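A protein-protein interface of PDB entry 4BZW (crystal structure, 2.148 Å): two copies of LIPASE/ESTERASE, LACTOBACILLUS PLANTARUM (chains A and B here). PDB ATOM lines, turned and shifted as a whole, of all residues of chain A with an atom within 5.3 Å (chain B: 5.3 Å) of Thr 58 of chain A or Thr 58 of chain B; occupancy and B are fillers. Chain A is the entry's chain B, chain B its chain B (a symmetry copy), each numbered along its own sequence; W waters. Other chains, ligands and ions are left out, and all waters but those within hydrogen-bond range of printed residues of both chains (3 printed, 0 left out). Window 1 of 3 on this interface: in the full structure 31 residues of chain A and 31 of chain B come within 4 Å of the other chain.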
ATOM      1  N   MET A   1      22.800  19.247  12.865  1.00  0.00           N
ATOM      2  CA  MET A   1      23.179  20.433  13.626  1.00  0.00           C
ATOM      3  C   MET A   1      24.167  20.078  14.736  1.00  0.00           C
ATOM      4  O   MET A   1      24.004  19.055  15.411  1.00  0.00           O
ATOM      5  CB  MET A   1      21.943  21.079  14.223  1.00  0.00           C
ATOM      6  CG  MET A   1      22.223  22.398  14.883  1.00  0.00           C
ATOM      7  SD  MET A   1      20.784  22.875  15.832  1.00  0.00           S
ATOM      8  CE  MET A   1      19.472  22.397  14.719  1.00  0.00           C
ATOM      9  N   GLU A  53      20.615  36.006  21.837  1.00  0.00           N
ATOM     10  CA  GLU A  53      21.597  35.004  21.426  1.00  0.00           C
ATOM     11  C   GLU A  53      20.933  33.826  20.701  1.00  0.00           C
ATOM     12  O   GLU A  53      20.549  33.954  19.543  1.00  0.00           O
ATOM     13  CB  GLU A  53      22.455  34.556  22.625  1.00  0.00           C
ATOM     14  CG  GLU A  53      23.302  35.710  23.201  1.00  0.00           C
ATOM     15  CD  GLU A  53      24.062  35.335  24.464  1.00  0.00           C
ATOM     16  OE1 GLU A  53      23.581  34.473  25.236  1.00  0.00           O
ATOM     17  OE2 GLU A  53      25.144  35.914  24.688  1.00  0.00           O
ATOM     18  N   ALA A  54      20.780  32.695  21.383  1.00  0.00           N
ATOM     19  CA  ALA A  54      20.165  31.509  20.772  1.00  0.00           C
ATOM     20  C   ALA A  54      18.790  31.719  20.087  1.00  0.00           C
ATOM     21  O   ALA A  54      18.562  31.179  19.001  1.00  0.00           O
ATOM     22  CB  ALA A  54      20.107  30.350  21.776  1.00  0.00           C
ATOM     23  N   PRO A  55      17.872  32.492  20.704  1.00  0.00           N
ATOM     24  CA  PRO A  55      16.583  32.694  20.014  1.00  0.00           C
ATOM     25  C   PRO A  55      16.723  33.303  18.615  1.00  0.00           C
ATOM     26  O   PRO A  55      16.033  32.887  17.672  1.00  0.00           O
ATOM     27  CB  PRO A  55      15.855  33.687  20.924  1.00  0.00           C
ATOM     28  CG  PRO A  55      16.407  33.430  22.301  1.00  0.00           C
ATOM     29  CD  PRO A  55      17.867  33.068  22.068  1.00  0.00           C
ATOM     30  N   ILE A  56      17.609  34.284  18.484  1.00  0.00           N
ATOM     31  CA  ILE A  56      17.848  34.923  17.191  1.00  0.00           C
ATOM     32  C   ILE A  56      18.659  34.012  16.265  1.00  0.00           C
ATOM     33  O   ILE A  56      18.338  33.866  15.081  1.00  0.00           O
ATOM     34  CB  ILE A  56      18.497  36.315  17.372  1.00  0.00           C
ATOM     35  CG1 ILE A  56      17.473  37.255  18.035  1.00  0.00           C
ATOM     36  CG2 ILE A  56      18.953  36.880  16.030  1.00  0.00           C
ATOM     37  CD1 ILE A  56      18.004  38.611  18.402  1.00  0.00           C
ATOM     38  N   ALA A  57      19.677  33.359  16.819  1.00  0.00           N
ATOM     39  CA  ALA A  57      20.504  32.431  16.051  1.00  0.00           C
ATOM     40  C   ALA A  57      19.664  31.299  15.448  1.00  0.00           C
ATOM     41  O   ALA A  57      19.818  30.943  14.279  1.00  0.00           O
ATOM     42  CB  ALA A  57      21.619  31.874  16.934  1.00  0.00           C
ATOM     43  N   THR A  58      18.767  30.741  16.253  1.00  0.00           N
ATOM     44  CA  THR A  58      17.900  29.651  15.798  1.00  0.00           C
ATOM     45  C   THR A  58      16.972  30.078  14.666  1.00  0.00           C
ATOM     46  O   THR A  58      16.786  29.331  13.692  1.00  0.00           O
ATOM     47  CB  THR A  58      17.100  29.054  16.970  1.00  0.00           C
ATOM     48  OG1 THR A  58      18.022  28.668  17.996  1.00  0.00           O
ATOM     49  CG2 THR A  58      16.321  27.817  16.532  1.00  0.00           C
ATOM     50  N   ARG A  59      16.399  31.281  14.774  1.00  0.00           N
ATOM     51  CA  ARG A  59      15.535  31.798  13.709  1.00  0.00           C
ATOM     52  C   ARG A  59      16.307  31.975  12.404  1.00  0.00           C
ATOM     53  O   ARG A  59      15.790  31.685  11.316  1.00  0.00           O
ATOM     54  CB  ARG A  59      14.885  33.130  14.118  1.00  0.00           C
ATOM     55  CG  ARG A  59      13.957  33.709  13.038  1.00  0.00           C
ATOM     56  CD  ARG A  59      12.858  32.708  12.688  1.00  0.00           C
ATOM     57  NE  ARG A  59      11.999  33.153  11.592  1.00  0.00           N
ATOM     58  CZ  ARG A  59      12.166  32.802  10.317  1.00  0.00           C
ATOM     59  NH1 ARG A  59      13.172  32.002   9.966  1.00  0.00           N
ATOM     60  NH2 ARG A  59      11.329  33.250   9.390  1.00  0.00           N
ATOM     61  N   MET A  60      17.541  32.465  12.508  1.00  0.00           N
ATOM     62  CA  MET A  60      18.381  32.621  11.325  1.00  0.00           C
ATOM     63  C   MET A  60      18.827  31.259  10.776  1.00  0.00           C
ATOM     64  O   MET A  60      18.901  31.071   9.564  1.00  0.00           O
ATOM     65  CB  MET A  60      19.579  33.532  11.623  1.00  0.00           C
ATOM     66  CG  MET A  60      19.185  34.952  12.021  1.00  0.00           C
ATOM     67  SD  MET A  60      18.116  35.773  10.824  1.00  0.00           S
ATOM     68  CE  MET A  60      17.672  37.225  11.779  1.00  0.00           C
ATOM     69  N   MET A  61      19.102  30.302  11.662  1.00  0.00           N
ATOM     70  CA  MET A  61      19.489  28.962  11.218  1.00  0.00           C
ATOM     71  C   MET A  61      18.374  28.263  10.440  1.00  0.00           C
ATOM     72  O   MET A  61      18.639  27.454   9.546  1.00  0.00           O
ATOM     73  CB  MET A  61      19.875  28.089  12.407  1.00  0.00           C
ATOM     74  CG  MET A  61      21.308  28.221  12.844  1.00  0.00           C
ATOM     75  SD  MET A  61      21.662  27.022  14.139  1.00  0.00           S
ATOM     76  CE  MET A  61      21.127  25.523  13.351  1.00  0.00           C
ATOM     77  N   ALA A  62      17.130  28.572  10.797  1.00  0.00           N
ATOM     78  CA  ALA A  62      15.965  27.962  10.156  1.00  0.00           C
ATOM     79  C   ALA A  62      15.877  28.369   8.692  1.00  0.00           C
ATOM     80  O   ALA A  62      15.200  27.718   7.897  1.00  0.00           O
ATOM     81  CB  ALA A  62      14.693  28.352  10.892  1.00  0.00           C
ATOM     82  N   THR A  67      25.414  29.877  12.391  1.00  0.00           N
ATOM     83  CA  THR A  67      25.481  31.065  13.244  1.00  0.00           C
ATOM     84  C   THR A  67      26.556  30.947  14.315  1.00  0.00           C
ATOM     85  O   THR A  67      26.908  29.846  14.734  1.00  0.00           O
ATOM     86  CB  THR A  67      24.129  31.397  13.938  1.00  0.00           C
ATOM     87  OG1 THR A  67      23.717  30.288  14.746  1.00  0.00           O
ATOM     88  CG2 THR A  67      23.041  31.725  12.906  1.00  0.00           C
ATOM     89  N   MET B   1      21.113  26.005  23.320  1.00  0.00           N
ATOM     90  CA  MET B   1      20.707  24.840  22.543  1.00  0.00           C
ATOM     91  C   MET B   1      21.695  23.689  22.725  1.00  0.00           C
ATOM     92  O   MET B   1      22.912  23.908  22.738  1.00  0.00           O
ATOM     93  CB  MET B   1      20.610  25.209  21.074  1.00  0.00           C
ATOM     94  CG  MET B   1      20.037  24.112  20.224  1.00  0.00           C
ATOM     95  SD  MET B   1      20.299  24.532  18.505  1.00  0.00           S
ATOM     96  CE  MET B   1      19.942  26.281  18.527  1.00  0.00           C
ATOM     97  N   GLU B  53      14.245  16.143   8.432  1.00  0.00           N
ATOM     98  CA  GLU B  53      14.735  16.023   9.804  1.00  0.00           C
ATOM     99  C   GLU B  53      15.160  17.383  10.372  1.00  0.00           C
ATOM    100  O   GLU B  53      14.309  18.196  10.723  1.00  0.00           O
ATOM    101  CB  GLU B  53      15.852  14.966   9.897  1.00  0.00           C
ATOM    102  CG  GLU B  53      15.348  13.551   9.545  1.00  0.00           C
ATOM    103  CD  GLU B  53      16.452  12.506   9.501  1.00  0.00           C
ATOM    104  OE1 GLU B  53      17.610  12.851   9.172  1.00  0.00           O
ATOM    105  OE2 GLU B  53      16.154  11.329   9.789  1.00  0.00           O
ATOM    106  N   ALA B  54      16.462  17.639  10.442  1.00  0.00           N
ATOM    107  CA  ALA B  54      16.966  18.909  10.981  1.00  0.00           C
ATOM    108  C   ALA B  54      16.366  20.205  10.375  1.00  0.00           C
ATOM    109  O   ALA B  54      16.071  21.143  11.117  1.00  0.00           O
ATOM    110  CB  ALA B  54      18.501  18.944  10.941  1.00  0.00           C
ATOM    111  N   PRO B  55      16.185  20.268   9.040  1.00  0.00           N
ATOM    112  CA  PRO B  55      15.588  21.503   8.496  1.00  0.00           C
ATOM    113  C   PRO B  55      14.213  21.835   9.088  1.00  0.00           C
ATOM    114  O   PRO B  55      13.919  23.001   9.387  1.00  0.00           O
ATOM    115  CB  PRO B  55      15.430  21.185   7.006  1.00  0.00           C
ATOM    116  CG  PRO B  55      16.519  20.192   6.702  1.00  0.00           C
ATOM    117  CD  PRO B  55      16.636  19.352   7.967  1.00  0.00           C
ATOM    118  N   ILE B  56      13.381  20.813   9.254  1.00  0.00           N
ATOM    119  CA  ILE B  56      12.053  21.004   9.834  1.00  0.00           C
ATOM    120  C   ILE B  56      12.138  21.232  11.346  1.00  0.00           C
ATOM    121  O   ILE B  56      11.480  22.124  11.890  1.00  0.00           O
ATOM    122  CB  ILE B  56      11.112  19.835   9.463  1.00  0.00           C
ATOM    123  CG1 ILE B  56      10.833  19.886   7.949  1.00  0.00           C
ATOM    124  CG2 ILE B  56       9.807  19.916  10.250  1.00  0.00           C
ATOM    125  CD1 ILE B  56      10.042  18.729   7.411  1.00  0.00           C
ATOM    126  N   ALA B  57      12.990  20.460  12.015  1.00  0.00           N
ATOM    127  CA  ALA B  57      13.192  20.605  13.455  1.00  0.00           C
ATOM    128  C   ALA B  57      13.660  22.019  13.816  1.00  0.00           C
ATOM    129  O   ALA B  57      13.169  22.632  14.765  1.00  0.00           O
ATOM    130  CB  ALA B  57      14.185  19.555  13.951  1.00  0.00           C
ATOM    131  N   THR B  58      14.612  22.536  13.047  1.00  0.00           N
ATOM    132  CA  THR B  58      15.146  23.879  13.285  1.00  0.00           C
ATOM    133  C   THR B  58      14.089  24.965  13.118  1.00  0.00           C
ATOM    134  O   THR B  58      14.022  25.904  13.927  1.00  0.00           O
ATOM    135  CB  THR B  58      16.365  24.157  12.387  1.00  0.00           C
ATOM    136  OG1 THR B  58      17.323  23.111  12.589  1.00  0.00           O
ATOM    137  CG2 THR B  58      17.022  25.487  12.745  1.00  0.00           C
ATOM    138  N   ARG B  59      13.248  24.839  12.086  1.00  0.00           N
ATOM    139  CA  ARG B  59      12.165  25.806  11.879  1.00  0.00           C
ATOM    140  C   ARG B  59      11.178  25.792  13.044  1.00  0.00           C
ATOM    141  O   ARG B  59      10.692  26.846  13.475  1.00  0.00           O
ATOM    142  CB  ARG B  59      11.424  25.533  10.560  1.00  0.00           C
ATOM    143  CG  ARG B  59      10.285  26.529  10.288  1.00  0.00           C
ATOM    144  CD  ARG B  59      10.821  27.959  10.270  1.00  0.00           C
ATOM    145  NE  ARG B  59       9.772  28.967  10.119  1.00  0.00           N
ATOM    146  CZ  ARG B  59       9.208  29.621  11.135  1.00  0.00           C
ATOM    147  NH1 ARG B  59       9.583  29.369  12.388  1.00  0.00           N
ATOM    148  NH2 ARG B  59       8.268  30.527  10.899  1.00  0.00           N
ATOM    149  N   MET B  60      10.870  24.598  13.543  1.00  0.00           N
ATOM    150  CA  MET B  60       9.978  24.480  14.692  1.00  0.00           C
ATOM    151  C   MET B  60      10.652  24.989  15.975  1.00  0.00           C
ATOM    152  O   MET B  60      10.005  25.614  16.811  1.00  0.00           O
ATOM    153  CB  MET B  60       9.475  23.039  14.850  1.00  0.00           C
ATOM    154  CG  MET B  60       8.659  22.542  13.660  1.00  0.00           C
ATOM    155  SD  MET B  60       7.261  23.600  13.244  1.00  0.00           S
ATOM    156  CE  MET B  60       6.783  22.852  11.686  1.00  0.00           C
ATOM    157  N   MET B  61      11.954  24.745  16.120  1.00  0.00           N
ATOM    158  CA  MET B  61      12.680  25.236  17.292  1.00  0.00           C
ATOM    159  C   MET B  61      12.709  26.763  17.358  1.00  0.00           C
ATOM    160  O   MET B  61      12.740  27.347  18.446  1.00  0.00           O
ATOM    161  CB  MET B  61      14.116  24.722  17.292  1.00  0.00           C
ATOM    162  CG  MET B  61      14.294  23.362  17.909  1.00  0.00           C
ATOM    163  SD  MET B  61      16.047  22.957  17.991  1.00  0.00           S
ATOM    164  CE  MET B  61      16.673  24.386  18.839  1.00  0.00           C
ATOM    165  N   ALA B  62      12.712  27.399  16.190  1.00  0.00           N
ATOM    166  CA  ALA B  62      12.762  28.859  16.101  1.00  0.00           C
ATOM    167  C   ALA B  62      11.499  29.481  16.684  1.00  0.00           C
ATOM    168  O   ALA B  62      11.478  30.663  17.022  1.00  0.00           O
ATOM    169  CB  ALA B  62      12.949  29.295  14.657  1.00  0.00           C
ATOM    170  N   THR B  67      12.727  19.772  20.023  1.00  0.00           N
ATOM    171  CA  THR B  67      12.380  18.797  18.986  1.00  0.00           C
ATOM    172  C   THR B  67      13.164  17.500  19.129  1.00  0.00           C
ATOM    173  O   THR B  67      14.270  17.489  19.664  1.00  0.00           O
ATOM    174  CB  THR B  67      12.586  19.339  17.543  1.00  0.00           C
ATOM    175  OG1 THR B  67      13.956  19.718  17.360  1.00  0.00           O
ATOM    176  CG2 THR B  67      11.669  20.538  17.264  1.00  0.00           C
HETATM  177  O   HOH W   1       8.270  33.053   9.146  1.00  0.00           O
HETATM  178  O   HOH W   2      15.492  24.908   8.648  1.00  0.00           O
HETATM  179  O   HOH W   3      14.098  31.255  18.175  1.00  0.00           O
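SD of Met 1 of chain A sits close to SD of Met 1 of chain B, 3.2 Å away.
The backbone carbonyl oxygen of Ala 54 of chain A sits at hydrogen-bond distance from the side-chain hydroxyl of Thr 58 of chain A, at 2.8 Å. The backbone carbonyl oxygen (O) of Ala 54 of chain B lies within hydrogen-bond range of the side-chain hydroxyl (OG1) of Thr 58 of chain B (2.8 Å).
Met 1 of chain A touches Thr 58 of chain B. Met 1 of chain B touches Thr 58 of chain A (CE to OG1, 3.1 Å). Thr 58 of chain B touches Thr 58 of chain A. Thr 58 of chain A touches Met 61 of chain B. Ala 62 of chain B touches Thr 58 of chain A (N to CG2, 3.6 Å). Arg 59 of chain A touches Ala 62 of chain B (CA to CB, 3.7 Å). C of Met 61 of chain A touches CG2 of Thr 58 of chain B (3.9 Å). Thr 58 of chain B touches Ala 62 of chain A. Ala 62 of chain A touches Arg 59 of chain B.
Glu 53 of chain A touches none of the printed residues of chain B. Of chain B, only Met 1 (3.1 Å), Thr 58 (3.97 Å), Met 61 (3.9 Å) and Ala 62 (3.6 Å) come within 4 Å of Thr 58 of chain A. Of the printed residues of chain B, Arg 59 of chain A touches Ala 62. Of the printed residues of chain A, Met 1 of chain B touches Met 1 (3.2 Å) and Thr 58 (3.1 Å). Of chain A, only Met 1 (3.1 Å), Thr 58 (3.97 Å), Met 61 (3.9 Å) and Ala 62 (3.7 Å) come within 4 Å of Thr 58 of chain B. Of the printed residues of chain A, Arg 59 of chain B touches Ala 62 (3.7 Å). Of the printed residues of chain A, Met 61 of chain B touches Thr 58 (3.9 Å). Of the printed residues of chain A, Ala 62 of chain B touches Thr 58 and Arg 59. The nearest printed residue of chain B that does not touch Thr 58 of chain A is Arg 59 of chain B (5.9 Å). The nearest printed residue of chain B that does not touch Met 1 of chain A is Ala 54 of chain B (4.7 Å).
Of the 12 printed residues of chain A, 5 touch a printed residue of chain B. Hydrophobic or aromatic side chains of chain A within 4 Å of the printed part of chain B: Met 1, Met 61 and Ala 62. Printed residues of chain B that touch a printed residue of chain A: Met 1, Thr 58, Arg 59, Met 61 and Ala 62. Hydrophobic or aromatic side chains of chain B within 4 Å of the printed part of chain A: Met 1, Met 61 and Ala 62. Among the printed residues, 10 pairs touch across the chains.
Met 1 of chain A touches its own counterpart, Met 1 of chain B. Thr 58 of chain A touches Met 61 of chain B, and with the chains exchanged Met 61 of chain A touches Thr 58 of chain B. Thr 58 of chain A touches Ala 62 of chain B, and with the chains exchanged Ala 62 of chain A touches Thr 58 of chain B. Arg 59 of chain A touches Ala 62 of chain B, and with the chains exchanged Ala 62 of chain A touches Arg 59 of chain B.
Water W2 bridges the backbone carbonyl oxygen of Pro 55 of chain B and the backbone carbonyl oxygen of Ala 62 of chain A. Water W3 lies within hydrogen-bond range of the backbone carbonyl oxygen of Pro 55 of chain A (2.6 Å) and the backbone carbonyl oxygen of Ala 62 of chain B (2.9 Å). Water W1 bridges the guanidinium group of Arg 59 of chain A (3.1 Å) and the guanidinium group of Arg 59 of chain B (3.1 Å).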
